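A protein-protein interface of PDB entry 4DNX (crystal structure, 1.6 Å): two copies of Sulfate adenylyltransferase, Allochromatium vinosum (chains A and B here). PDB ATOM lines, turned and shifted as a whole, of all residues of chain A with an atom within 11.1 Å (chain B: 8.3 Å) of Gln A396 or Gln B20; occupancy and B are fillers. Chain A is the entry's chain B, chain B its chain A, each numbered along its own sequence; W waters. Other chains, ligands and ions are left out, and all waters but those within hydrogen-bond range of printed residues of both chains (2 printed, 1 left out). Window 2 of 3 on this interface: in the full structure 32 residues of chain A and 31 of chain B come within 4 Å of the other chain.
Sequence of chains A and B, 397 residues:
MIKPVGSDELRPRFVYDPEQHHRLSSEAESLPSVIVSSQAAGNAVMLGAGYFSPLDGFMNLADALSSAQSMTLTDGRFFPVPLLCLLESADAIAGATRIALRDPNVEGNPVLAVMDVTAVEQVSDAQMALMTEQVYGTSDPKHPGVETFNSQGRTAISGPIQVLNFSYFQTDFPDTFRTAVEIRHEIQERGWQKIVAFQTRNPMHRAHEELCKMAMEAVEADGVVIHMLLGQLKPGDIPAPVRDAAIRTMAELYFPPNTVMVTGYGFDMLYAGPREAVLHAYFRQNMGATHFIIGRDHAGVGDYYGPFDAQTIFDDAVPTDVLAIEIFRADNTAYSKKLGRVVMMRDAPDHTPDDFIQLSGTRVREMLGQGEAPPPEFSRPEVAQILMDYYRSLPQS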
ATOM      1  N   THR A 171     -21.940   3.416  19.489  1.00  0.00           N
ATOM      2  CA  THR A 171     -21.607   1.999  19.644  1.00  0.00           C
ATOM      3  C   THR A 171     -22.027   1.125  18.461  1.00  0.00           C
ATOM      4  O   THR A 171     -21.255   0.264  17.979  1.00  0.00           O
ATOM      5  CB  THR A 171     -22.283   1.445  20.941  1.00  0.00           C
ATOM      6  OG1 THR A 171     -21.836   2.243  22.036  1.00  0.00           O
ATOM      7  CG2 THR A 171     -21.868  -0.026  21.196  1.00  0.00           C
ATOM      8  N   ASP A 172     -23.252   1.359  17.999  1.00  0.00           N
ATOM      9  CA  ASP A 172     -23.825   0.545  16.926  1.00  0.00           C
ATOM     10  C   ASP A 172     -23.422   1.001  15.538  1.00  0.00           C
ATOM     11  O   ASP A 172     -23.442   0.195  14.594  1.00  0.00           O
ATOM     12  CB  ASP A 172     -25.351   0.544  17.018  1.00  0.00           C
ATOM     13  CG  ASP A 172     -25.881  -0.239  18.220  1.00  0.00           C
ATOM     14  OD1 ASP A 172     -25.089  -0.731  19.060  1.00  0.00           O
ATOM     15  OD2 ASP A 172     -27.123  -0.311  18.340  1.00  0.00           O
ATOM     16  N   PHE A 173     -23.075   2.280  15.403  1.00  0.00           N
ATOM     17  CA  PHE A 173     -22.764   2.880  14.084  1.00  0.00           C
ATOM     18  C   PHE A 173     -21.427   3.664  14.136  1.00  0.00           C
ATOM     19  O   PHE A 173     -21.404   4.881  13.862  1.00  0.00           O
ATOM     20  CB  PHE A 173     -23.905   3.806  13.622  1.00  0.00           C
ATOM     21  CG  PHE A 173     -25.295   3.228  13.833  1.00  0.00           C
ATOM     22  CD1 PHE A 173     -25.824   2.316  12.922  1.00  0.00           C
ATOM     23  CD2 PHE A 173     -26.086   3.643  14.904  1.00  0.00           C
ATOM     24  CE1 PHE A 173     -27.110   1.771  13.125  1.00  0.00           C
ATOM     25  CE2 PHE A 173     -27.354   3.110  15.136  1.00  0.00           C
ATOM     26  CZ  PHE A 173     -27.874   2.167  14.240  1.00  0.00           C
ATOM     27  N   LEU A 233     -33.847  -0.455  14.681  1.00  0.00           N
ATOM     28  CA  LEU A 233     -34.270  -1.166  13.484  1.00  0.00           C
ATOM     29  C   LEU A 233     -35.748  -1.553  13.605  1.00  0.00           C
ATOM     30  O   LEU A 233     -36.286  -1.618  14.714  1.00  0.00           O
ATOM     31  CB  LEU A 233     -33.408  -2.428  13.283  1.00  0.00           C
ATOM     32  CG  LEU A 233     -33.051  -3.225  14.547  1.00  0.00           C
ATOM     33  CD1 LEU A 233     -33.504  -4.682  14.453  1.00  0.00           C
ATOM     34  CD2 LEU A 233     -31.553  -3.132  14.856  1.00  0.00           C
ATOM     35  N   ASP A 237     -36.395  -3.859   7.575  1.00  0.00           N
ATOM     36  CA  ASP A 237     -35.380  -2.849   7.265  1.00  0.00           C
ATOM     37  C   ASP A 237     -34.149  -3.445   6.611  1.00  0.00           C
ATOM     38  O   ASP A 237     -33.713  -4.541   6.948  1.00  0.00           O
ATOM     39  CB  ASP A 237     -34.911  -2.133   8.538  1.00  0.00           C
ATOM     40  CG  ASP A 237     -35.597  -0.807   8.752  1.00  0.00           C
ATOM     41  OD1 ASP A 237     -36.237  -0.297   7.805  1.00  0.00           O
ATOM     42  OD2 ASP A 237     -35.493  -0.270   9.878  1.00  0.00           O
ATOM     43  N   ILE A 238     -33.564  -2.683   5.704  1.00  0.00           N
ATOM     44  CA  ILE A 238     -32.248  -3.003   5.170  1.00  0.00           C
ATOM     45  C   ILE A 238     -31.232  -2.700   6.312  1.00  0.00           C
ATOM     46  O   ILE A 238     -31.274  -1.597   6.854  1.00  0.00           O
ATOM     47  CB  ILE A 238     -32.017  -2.108   3.937  1.00  0.00           C
ATOM     48  CG1 ILE A 238     -30.554  -1.940   3.608  1.00  0.00           C
ATOM     49  CG2 ILE A 238     -32.659  -0.748   4.149  1.00  0.00           C
ATOM     50  CD1 ILE A 238     -30.359  -1.065   2.457  1.00  0.00           C
ATOM     51  N   PRO A 239     -30.333  -3.630   6.662  1.00  0.00           N
ATOM     52  CA  PRO A 239     -29.380  -3.317   7.760  1.00  0.00           C
ATOM     53  C   PRO A 239     -28.628  -2.011   7.501  1.00  0.00           C
ATOM     54  O   PRO A 239     -28.271  -1.706   6.341  1.00  0.00           O
ATOM     55  CB  PRO A 239     -28.392  -4.491   7.730  1.00  0.00           C
ATOM     56  CG  PRO A 239     -29.229  -5.673   7.182  1.00  0.00           C
ATOM     57  CD  PRO A 239     -30.078  -4.977   6.103  1.00  0.00           C
ATOM     58  N   ALA A 240     -28.335  -1.263   8.572  1.00  0.00           N
ATOM     59  CA  ALA A 240     -27.541  -0.060   8.432  1.00  0.00           C
ATOM     60  C   ALA A 240     -26.239  -0.181   7.602  1.00  0.00           C
ATOM     61  O   ALA A 240     -25.984   0.740   6.793  1.00  0.00           O
ATOM     62  CB  ALA A 240     -27.260   0.571   9.829  1.00  0.00           C
ATOM     63  N   PRO A 241     -25.412  -1.234   7.741  1.00  0.00           N
ATOM     64  CA  PRO A 241     -24.169  -1.248   6.958  1.00  0.00           C
ATOM     65  C   PRO A 241     -24.393  -1.413   5.450  1.00  0.00           C
ATOM     66  O   PRO A 241     -23.580  -0.939   4.665  1.00  0.00           O
ATOM     67  CB  PRO A 241     -23.365  -2.413   7.525  1.00  0.00           C
ATOM     68  CG  PRO A 241     -24.320  -3.218   8.346  1.00  0.00           C
ATOM     69  CD  PRO A 241     -25.451  -2.348   8.726  1.00  0.00           C
ATOM     70  N   VAL A 242     -25.482  -2.077   5.065  1.00  0.00           N
ATOM     71  CA  VAL A 242     -25.843  -2.212   3.642  1.00  0.00           C
ATOM     72  C   VAL A 242     -26.316  -0.858   3.072  1.00  0.00           C
ATOM     73  O   VAL A 242     -25.957  -0.467   1.941  1.00  0.00           O
ATOM     74  CB  VAL A 242     -26.955  -3.294   3.454  1.00  0.00           C
ATOM     75  CG1 VAL A 242     -27.452  -3.332   1.984  1.00  0.00           C
ATOM     76  CG2 VAL A 242     -26.460  -4.670   3.910  1.00  0.00           C
ATOM     77  N   ASP A 389     -26.955  -7.993  -3.731  1.00  0.00           N
ATOM     78  CA  ASP A 389     -25.999  -8.865  -3.027  1.00  0.00           C
ATOM     79  C   ASP A 389     -26.462  -9.160  -1.609  1.00  0.00           C
ATOM     80  O   ASP A 389     -26.338 -10.312  -1.147  1.00  0.00           O
ATOM     81  CB  ASP A 389     -24.569  -8.293  -3.019  1.00  0.00           C
ATOM     82  CG  ASP A 389     -23.871  -8.373  -4.410  1.00  0.00           C
ATOM     83  OD1 ASP A 389     -22.851  -7.689  -4.592  1.00  0.00           O
ATOM     84  OD2 ASP A 389     -24.339  -9.075  -5.329  1.00  0.00           O
ATOM     85  N   TYR A 390     -26.999  -8.148  -0.932  1.00  0.00           N
ATOM     86  CA  TYR A 390     -27.537  -8.326   0.403  1.00  0.00           C
ATOM     87  C   TYR A 390     -28.726  -9.298   0.351  1.00  0.00           C
ATOM     88  O   TYR A 390     -28.736 -10.298   1.071  1.00  0.00           O
ATOM     89  CB  TYR A 390     -27.894  -6.978   1.072  1.00  0.00           C
ATOM     90  CG  TYR A 390     -28.918  -7.150   2.160  1.00  0.00           C
ATOM     91  CD1 TYR A 390     -28.611  -7.831   3.351  1.00  0.00           C
ATOM     92  CD2 TYR A 390     -30.216  -6.688   1.979  1.00  0.00           C
ATOM     93  CE1 TYR A 390     -29.609  -8.033   4.346  1.00  0.00           C
ATOM     94  CE2 TYR A 390     -31.188  -6.867   2.957  1.00  0.00           C
ATOM     95  CZ  TYR A 390     -30.884  -7.539   4.120  1.00  0.00           C
ATOM     96  OH  TYR A 390     -31.894  -7.684   5.037  1.00  0.00           O
ATOM     97  N   TYR A 391     -29.707  -9.036  -0.512  1.00  0.00           N
ATOM     98  CA  TYR A 391     -30.906  -9.909  -0.562  1.00  0.00           C
ATOM     99  C   TYR A 391     -30.586 -11.362  -0.959  1.00  0.00           C
ATOM    100  O   TYR A 391     -31.263 -12.303  -0.536  1.00  0.00           O
ATOM    101  CB  TYR A 391     -31.997  -9.334  -1.485  1.00  0.00           C
ATOM    102  CG  TYR A 391     -32.612  -8.023  -1.038  1.00  0.00           C
ATOM    103  CD1 TYR A 391     -33.361  -7.921   0.140  1.00  0.00           C
ATOM    104  CD2 TYR A 391     -32.465  -6.882  -1.813  1.00  0.00           C
ATOM    105  CE1 TYR A 391     -33.932  -6.682   0.533  1.00  0.00           C
ATOM    106  CE2 TYR A 391     -33.011  -5.660  -1.444  1.00  0.00           C
ATOM    107  CZ  TYR A 391     -33.757  -5.556  -0.275  1.00  0.00           C
ATOM    108  OH  TYR A 391     -34.282  -4.313   0.054  1.00  0.00           O
ATOM    109  N   ARG A 392     -29.541 -11.560  -1.755  1.00  0.00           N
ATOM    110  CA  ARG A 392     -29.200 -12.912  -2.183  1.00  0.00           C
ATOM    111  C   ARG A 392     -28.201 -13.621  -1.247  1.00  0.00           C
ATOM    112  O   ARG A 392     -27.986 -14.828  -1.355  1.00  0.00           O
ATOM    113  CB  ARG A 392     -28.784 -12.911  -3.655  1.00  0.00           C
ATOM    114  CG  ARG A 392     -29.978 -12.531  -4.560  1.00  0.00           C
ATOM    115  CD  ARG A 392     -29.543 -12.127  -5.955  1.00  0.00           C
ATOM    116  NE  ARG A 392     -29.843 -13.187  -6.916  1.00  0.00           N
ATOM    117  CZ  ARG A 392     -29.167 -13.409  -8.042  1.00  0.00           C
ATOM    118  NH1 ARG A 392     -28.141 -12.633  -8.379  1.00  0.00           N
ATOM    119  NH2 ARG A 392     -29.525 -14.405  -8.840  1.00  0.00           N
ATOM    120  N   SER A 393     -27.631 -12.868  -0.306  1.00  0.00           N
ATOM    121  CA  SER A 393     -26.729 -13.436   0.708  1.00  0.00           C
ATOM    122  C   SER A 393     -27.480 -14.323   1.691  1.00  0.00           C
ATOM    123  O   SER A 393     -28.655 -14.056   2.041  1.00  0.00           O
ATOM    124  CB  SER A 393     -26.011 -12.339   1.490  1.00  0.00           C
ATOM    125  OG  SER A 393     -26.885 -11.723   2.442  1.00  0.00           O
ATOM    126  N   LEU A 394     -26.777 -15.368   2.133  1.00  0.00           N
ATOM    127  CA  LEU A 394     -27.259 -16.330   3.123  1.00  0.00           C
ATOM    128  C   LEU A 394     -27.788 -15.590   4.358  1.00  0.00           C
ATOM    129  O   LEU A 394     -27.056 -14.788   4.948  1.00  0.00           O
ATOM    130  CB  LEU A 394     -26.118 -17.293   3.501  1.00  0.00           C
ATOM    131  CG  LEU A 394     -26.365 -18.774   3.848  1.00  0.00           C
ATOM    132  CD1 LEU A 394     -26.454 -18.957   5.362  1.00  0.00           C
ATOM    133  CD2 LEU A 394     -27.580 -19.414   3.124  1.00  0.00           C
ATOM    134  N   PRO A 395     -29.053 -15.829   4.727  1.00  0.00           N
ATOM    135  CA  PRO A 395     -29.656 -15.141   5.887  1.00  0.00           C
ATOM    136  C   PRO A 395     -28.945 -15.426   7.226  1.00  0.00           C
ATOM    137  O   PRO A 395     -28.331 -16.496   7.389  1.00  0.00           O
ATOM    138  CB  PRO A 395     -31.089 -15.696   5.914  1.00  0.00           C
ATOM    139  CG  PRO A 395     -31.377 -16.015   4.484  1.00  0.00           C
ATOM    140  CD  PRO A 395     -30.077 -16.545   3.933  1.00  0.00           C
ATOM    141  N   GLN A 396     -29.043 -14.465   8.154  1.00  0.00           N
ATOM    142  CA  GLN A 396     -28.500 -14.550   9.526  1.00  0.00           C
ATOM    143  C   GLN A 396     -27.030 -14.131   9.604  1.00  0.00           C
ATOM    144  O   GLN A 396     -26.715 -13.043  10.097  1.00  0.00           O
ATOM    145  CB  GLN A 396     -28.759 -15.930  10.186  1.00  0.00           C
ATOM    146  CG  GLN A 396     -27.512 -16.659  10.721  1.00  0.00           C
ATOM    147  CD  GLN A 396     -27.672 -17.199  12.153  1.00  0.00           C
ATOM    148  OE1 GLN A 396     -27.583 -18.405  12.381  1.00  0.00           O
ATOM    149  NE2 GLN A 396     -27.882 -16.301  13.118  1.00  0.00           N
ATOM    150  N   VAL B  15     -18.850  -6.280  14.838  1.00  0.00           N
ATOM    151  CA  VAL B  15     -20.200  -6.709  14.389  1.00  0.00           C
ATOM    152  C   VAL B  15     -20.975  -5.462  13.896  1.00  0.00           C
ATOM    153  O   VAL B  15     -21.756  -4.822  14.634  1.00  0.00           O
ATOM    154  CB  VAL B  15     -20.952  -7.427  15.500  1.00  0.00           C
ATOM    155  CG1 VAL B  15     -22.324  -7.976  14.966  1.00  0.00           C
ATOM    156  CG2 VAL B  15     -20.081  -8.570  16.001  1.00  0.00           C
ATOM    157  N   TYR B  16     -20.813  -5.162  12.606  1.00  0.00           N
ATOM    158  CA  TYR B  16     -21.500  -4.005  11.991  1.00  0.00           C
ATOM    159  C   TYR B  16     -23.039  -4.075  11.902  1.00  0.00           C
ATOM    160  O   TYR B  16     -23.687  -3.035  11.910  1.00  0.00           O
ATOM    161  CB  TYR B  16     -20.951  -3.721  10.591  1.00  0.00           C
ATOM    162  CG  TYR B  16     -19.658  -2.944  10.570  1.00  0.00           C
ATOM    163  CD1 TYR B  16     -19.652  -1.549  10.720  1.00  0.00           C
ATOM    164  CD2 TYR B  16     -18.435  -3.611  10.412  1.00  0.00           C
ATOM    165  CE1 TYR B  16     -18.459  -0.831  10.730  1.00  0.00           C
ATOM    166  CE2 TYR B  16     -17.206  -2.884  10.399  1.00  0.00           C
ATOM    167  CZ  TYR B  16     -17.258  -1.485  10.519  1.00  0.00           C
ATOM    168  OH  TYR B  16     -16.108  -0.749  10.513  1.00  0.00           O
ATOM    169  N   ASP B  17     -23.628  -5.278  11.801  1.00  0.00           N
ATOM    170  CA  ASP B  17     -25.067  -5.413  11.716  1.00  0.00           C
ATOM    171  C   ASP B  17     -25.650  -5.187  13.117  1.00  0.00           C
ATOM    172  O   ASP B  17     -25.329  -5.966  14.009  1.00  0.00           O
ATOM    173  CB  ASP B  17     -25.417  -6.824  11.239  1.00  0.00           C
ATOM    174  CG  ASP B  17     -26.913  -7.032  11.101  1.00  0.00           C
ATOM    175  OD1 ASP B  17     -27.528  -6.296  10.321  1.00  0.00           O
ATOM    176  OD2 ASP B  17     -27.476  -7.931  11.765  1.00  0.00           O
ATOM    177  N   PRO B  18     -26.470  -4.151  13.327  1.00  0.00           N
ATOM    178  CA  PRO B  18     -26.937  -3.827  14.682  1.00  0.00           C
ATOM    179  C   PRO B  18     -27.794  -4.943  15.305  1.00  0.00           C
ATOM    180  O   PRO B  18     -27.694  -5.168  16.498  1.00  0.00           O
ATOM    181  CB  PRO B  18     -27.766  -2.561  14.488  1.00  0.00           C
ATOM    182  CG  PRO B  18     -27.148  -1.926  13.307  1.00  0.00           C
ATOM    183  CD  PRO B  18     -26.654  -3.004  12.408  1.00  0.00           C
ATOM    184  N   GLU B  19     -28.602  -5.635  14.508  1.00  0.00           N
ATOM    185  CA  GLU B  19     -29.425  -6.709  15.078  1.00  0.00           C
ATOM    186  C   GLU B  19     -28.565  -7.861  15.612  1.00  0.00           C
ATOM    187  O   GLU B  19     -28.793  -8.353  16.739  1.00  0.00           O
ATOM    188  CB  GLU B  19     -30.472  -7.196  14.075  1.00  0.00           C
ATOM    189  CG  GLU B  19     -31.238  -8.364  14.620  1.00  0.00           C
ATOM    190  CD  GLU B  19     -32.651  -8.437  14.111  1.00  0.00           C
ATOM    191  OE1 GLU B  19     -32.830  -8.873  12.952  1.00  0.00           O
ATOM    192  OE2 GLU B  19     -33.579  -8.072  14.873  1.00  0.00           O
ATOM    193  N   GLN B  20     -27.569  -8.283  14.832  1.00  0.00           N
ATOM    194  CA  GLN B  20     -26.587  -9.310  15.263  1.00  0.00           C
ATOM    195  C   GLN B  20     -25.748  -8.840  16.470  1.00  0.00           C
ATOM    196  O   GLN B  20     -25.497  -9.598  17.412  1.00  0.00           O
ATOM    197  CB  GLN B  20     -25.637  -9.671  14.113  1.00  0.00           C
ATOM    198  CG  GLN B  20     -26.247 -10.628  13.055  1.00  0.00           C
ATOM    199  CD  GLN B  20     -26.831 -11.918  13.667  1.00  0.00           C
ATOM    200  OE1 GLN B  20     -28.002 -12.261  13.439  1.00  0.00           O
ATOM    201  NE2 GLN B  20     -26.017 -12.621  14.464  1.00  0.00           N
ATOM    202  N   HIS B  21     -25.343  -7.575  16.437  1.00  0.00           N
ATOM    203  CA  HIS B  21     -24.685  -6.950  17.605  1.00  0.00           C
ATOM    204  C   HIS B  21     -25.493  -7.063  18.900  1.00  0.00           C
ATOM    205  O   HIS B  21     -24.960  -7.509  19.957  1.00  0.00           O
ATOM    206  CB  HIS B  21     -24.430  -5.472  17.274  1.00  0.00           C
ATOM    207  CG  HIS B  21     -23.581  -4.740  18.271  1.00  0.00           C
ATOM    208  ND1 HIS B  21     -22.951  -3.555  17.952  1.00  0.00           N
ATOM    209  CD2 HIS B  21     -23.317  -4.959  19.588  1.00  0.00           C
ATOM    210  CE1 HIS B  21     -22.277  -3.109  19.006  1.00  0.00           C
ATOM    211  NE2 HIS B  21     -22.498  -3.929  20.019  1.00  0.00           N
ATOM    212  N   HIS B  22     -26.776  -6.715  18.821  1.00  0.00           N
ATOM    213  CA  HIS B  22     -27.661  -6.784  20.003  1.00  0.00           C
ATOM    214  C   HIS B  22     -27.815  -8.223  20.476  1.00  0.00           C
ATOM    215  O   HIS B  22     -27.775  -8.493  21.677  1.00  0.00           O
ATOM    216  CB  HIS B  22     -29.047  -6.171  19.715  1.00  0.00           C
ATOM    217  CG  HIS B  22     -29.001  -4.740  19.262  1.00  0.00           C
ATOM    218  ND1 HIS B  22     -30.047  -4.144  18.585  1.00  0.00           N
ATOM    219  CD2 HIS B  22     -28.040  -3.790  19.396  1.00  0.00           C
ATOM    220  CE1 HIS B  22     -29.731  -2.885  18.320  1.00  0.00           C
ATOM    221  NE2 HIS B  22     -28.511  -2.654  18.779  1.00  0.00           N
ATOM    222  N   ARG B  23     -27.966  -9.154  19.533  1.00  0.00           N
ATOM    223  CA  ARG B  23     -28.102 -10.572  19.916  1.00  0.00           C
ATOM    224  C   ARG B  23     -26.842 -11.119  20.610  1.00  0.00           C
ATOM    225  O   ARG B  23     -26.956 -11.868  21.618  1.00  0.00           O
ATOM    226  CB  ARG B  23     -28.441 -11.425  18.699  1.00  0.00           C
ATOM    227  CG  ARG B  23     -29.886 -11.227  18.271  1.00  0.00           C
ATOM    228  CD  ARG B  23     -30.143 -11.619  16.818  1.00  0.00           C
ATOM    229  NE  ARG B  23     -30.019 -13.055  16.614  1.00  0.00           N
ATOM    230  CZ  ARG B  23     -31.031 -13.918  16.653  1.00  0.00           C
ATOM    231  NH1 ARG B  23     -32.268 -13.497  16.902  1.00  0.00           N
ATOM    232  NH2 ARG B  23     -30.800 -15.208  16.456  1.00  0.00           N
ATOM    233  N   LEU B  24     -25.673 -10.749  20.079  1.00  0.00           N
ATOM    234  CA  LEU B  24     -24.396 -11.186  20.646  1.00  0.00           C
ATOM    235  C   LEU B  24     -24.158 -10.562  22.025  1.00  0.00           C
ATOM    236  O   LEU B  24     -23.678 -11.234  22.959  1.00  0.00           O
ATOM    237  CB  LEU B  24     -23.226 -10.856  19.697  1.00  0.00           C
ATOM    238  CG  LEU B  24     -23.153 -11.805  18.479  1.00  0.00           C
ATOM    239  CD1 LEU B  24     -22.082 -11.378  17.434  1.00  0.00           C
ATOM    240  CD2 LEU B  24     -22.888 -13.242  18.919  1.00  0.00           C
ATOM    241  N   SER B  25     -24.464  -9.271  22.143  1.00  0.00           N
ATOM    242  CA  SER B  25     -24.327  -8.581  23.439  1.00  0.00           C
ATOM    243  C   SER B  25     -25.191  -9.268  24.490  1.00  0.00           C
ATOM    244  O   SER B  25     -24.758  -9.472  25.644  1.00  0.00           O
ATOM    245  CB  SER B  25     -24.776  -7.123  23.336  1.00  0.00           C
ATOM    246  OG  SER B  25     -23.792  -6.439  22.630  1.00  0.00           O
ATOM    247  N   SER B  26     -26.414  -9.618  24.098  1.00  0.00           N
ATOM    248  CA  SER B  26     -27.318 -10.315  25.012  1.00  0.00           C
ATOM    249  C   SER B  26     -26.765 -11.668  25.413  1.00  0.00           C
ATOM    250  O   SER B  26     -26.773 -12.028  26.604  1.00  0.00           O
ATOM    251  CB  SER B  26     -28.692 -10.495  24.362  1.00  0.00           C
ATOM    252  OG  SER B  26     -29.438  -9.314  24.517  1.00  0.00           O
ATOM    253  N   GLU B  27     -26.288 -12.418  24.423  1.00  0.00           N
ATOM    254  CA  GLU B  27     -25.704 -13.750  24.644  1.00  0.00           C
ATOM    255  C   GLU B  27     -24.504 -13.686  25.575  1.00  0.00           C
ATOM    256  O   GLU B  27     -24.335 -14.565  26.430  1.00  0.00           O
ATOM    257  CB  GLU B  27     -25.233 -14.356  23.317  1.00  0.00           C
ATOM    258  CG  GLU B  27     -24.836 -15.825  23.415  1.00  0.00           C
ATOM    259  CD  GLU B  27     -24.184 -16.395  22.150  1.00  0.00           C
ATOM    260  OE1 GLU B  27     -24.084 -15.674  21.125  1.00  0.00           O
ATOM    261  OE2 GLU B  27     -23.749 -17.585  22.188  1.00  0.00           O
ATOM    262  N   ARG B  98     -17.393 -21.289  23.702  1.00  0.00           N
ATOM    263  CA  ARG B  98     -17.772 -19.922  23.369  1.00  0.00           C
ATOM    264  C   ARG B  98     -17.748 -19.137  24.688  1.00  0.00           C
ATOM    265  O   ARG B  98     -18.352 -19.584  25.692  1.00  0.00           O
ATOM    266  CB  ARG B  98     -19.170 -19.942  22.777  1.00  0.00           C
ATOM    267  CG  ARG B  98     -19.667 -18.658  22.229  1.00  0.00           C
ATOM    268  CD  ARG B  98     -20.725 -19.044  21.194  1.00  0.00           C
ATOM    269  NE  ARG B  98     -21.407 -17.874  20.695  1.00  0.00           N
ATOM    270  CZ  ARG B  98     -20.962 -17.129  19.689  1.00  0.00           C
ATOM    271  NH1 ARG B  98     -19.835 -17.448  19.066  1.00  0.00           N
ATOM    272  NH2 ARG B  98     -21.654 -16.065  19.300  1.00  0.00           N
ATOM    273  N   VAL B 114     -16.745 -11.570  21.761  1.00  0.00           N
ATOM    274  CA  VAL B 114     -17.152 -12.956  21.983  1.00  0.00           C
ATOM    275  C   VAL B 114     -16.165 -13.824  21.188  1.00  0.00           C
ATOM    276  O   VAL B 114     -15.840 -13.514  20.039  1.00  0.00           O
ATOM    277  CB  VAL B 114     -18.606 -13.162  21.466  1.00  0.00           C
ATOM    278  CG1 VAL B 114     -19.003 -14.628  21.549  1.00  0.00           C
ATOM    279  CG2 VAL B 114     -19.566 -12.332  22.282  1.00  0.00           C
ATOM    280  N   GLN B 162     -15.580 -12.033  17.578  1.00  0.00           N
ATOM    281  CA  GLN B 162     -16.551 -11.017  17.118  1.00  0.00           C
ATOM    282  C   GLN B 162     -16.459  -9.889  18.135  1.00  0.00           C
ATOM    283  O   GLN B 162     -16.741 -10.089  19.331  1.00  0.00           O
ATOM    284  CB  GLN B 162     -17.963 -11.608  17.078  1.00  0.00           C
ATOM    285  CG  GLN B 162     -18.085 -12.744  16.069  1.00  0.00           C
ATOM    286  CD  GLN B 162     -19.353 -13.590  16.292  1.00  0.00           C
ATOM    287  OE1 GLN B 162     -19.522 -14.286  17.322  1.00  0.00           O
ATOM    288  NE2 GLN B 162     -20.241 -13.522  15.345  1.00  0.00           N
ATOM    289  N   LEU B 164     -17.442  -6.248  19.842  1.00  0.00           N
ATOM    290  CA  LEU B 164     -18.695  -5.550  20.120  1.00  0.00           C
ATOM    291  C   LEU B 164     -18.526  -4.042  20.303  1.00  0.00           C
ATOM    292  O   LEU B 164     -19.489  -3.270  20.218  1.00  0.00           O
ATOM    293  CB  LEU B 164     -19.382  -6.163  21.367  1.00  0.00           C
ATOM    294  CG  LEU B 164     -19.734  -7.645  21.200  1.00  0.00           C
ATOM    295  CD1 LEU B 164     -20.501  -8.078  22.458  1.00  0.00           C
ATOM    296  CD2 LEU B 164     -20.601  -7.900  19.968  1.00  0.00           C
HETATM  297  O   HOH W   1     -23.088  -0.310  11.867  1.00  0.00           O
HETATM  298  O   HOH W   2     -29.401   0.194  17.076  1.00  0.00           O
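No position is printed for both chains. Of the 11 pairs that touch across the chains among the printed residues, none has its exchanged pair printed and touching as well.
A ring nitrogen (NE2) of His B22 sits at hydrogen-bond distance from the side-chain carboxylate (OD2) of Asp A172.
Water W2 bridges the side-chain carboxylate (OD2) of Asp A172 (2.7 Å) and a ring nitrogen (NE2) of His B22 (3.4 Å). Water W1 lies within hydrogen-bond range of the backbone carbonyl oxygen (O) of Tyr B16 and the backbone carbonyl oxygen (O) of Asp A172.
Of chain B, only Gln B20 comes within 4 Å of Gln A396. Of chain A, only Gln A396 comes within 4 Å of Gln B20. Of chain A, only Pro A239 comes within 4 Å of Asp B17. Pro B18 touches just these residues of chain A: Phe A173 (3.7 Å), Leu A233 (3.8 Å) and Pro A241 (3.9 Å). His B22 touches just these residues of chain A: Asp A172 (2.8 Å) and Leu A233 (3.9 Å). No residue of chain A comes within 4 Å of Arg B23. No residue of chain A comes within 4 Å of Leu B24. Of the printed residues of chain A, His B21 touches Thr A171 and Asp A172. Of the printed residues of chain B, Phe A173 touches Pro B18. Of the printed residues of chain B, Leu A233 touches Pro B18, Glu B19 and His B22. Of the printed residues of chain B, Pro A239 touches Asp B17 (3.3 Å). Of the printed residues of chain A, Tyr B16 touches Pro A241 (3.6 Å). Arg A392 touches none of the printed residues of chain B. The nearest residue of chain B that does not touch Gln A396 is Arg B23 (4.6 Å). The nearest residue of chain A that does not touch Gln B20 is Leu A233 (6.5 Å).
Of the 18 printed residues of chain A, 7 touch a printed residue of chain B. Printed residues of chain B that touch a printed residue of chain A: Tyr B16, Asp B17, Pro B18, Glu B19, Gln B20, His B21 and His B22. Hydrophobic or aromatic side chains of chain B that line the printed part of chain A: Pro B18, His B21 and His B22. Among the printed residues, no Asp or Glu carboxylate lies within 4 Å of a Lys or Arg side-chain nitrogen of the other chain.
Among the printed residues, merely in contact across the chains: Thr A171 with His B21 (3.7 Å), Asp A172 with His B21 (3.7 Å), Phe A173 with Pro B18 (3.7 Å), Leu A233 with Pro B18 (3.8 Å), Leu A233 with Glu B19 (3.4 Å), Leu A233 with His B22 (3.9 Å), Pro A239 with Asp B17 (3.3 Å), Pro A241 with Tyr B16 (3.6 Å), Pro A241 with Pro B18 (3.9 Å) and Gln A396 with Gln B20 (3.7 Å).
OD2 of Asp B17 is in hydrogen-bond range of N of Gln B20 (3.1 Å). The backbone carbonyl oxygen (O) of Pro B18 lies close to a ring nitrogen (ND1) of His B22. The side-chain hydroxyl of Ser B25 sits at hydrogen-bond distance from the backbone carbonyl oxygen of His B21 (3.1 Å). A ring nitrogen (NE2) of His B21 sits close to the backbone carbonyl oxygen (O) of Leu B164 (3.1 Å). OG of Ser B26 sits at hydrogen-bond distance from O of His B22.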
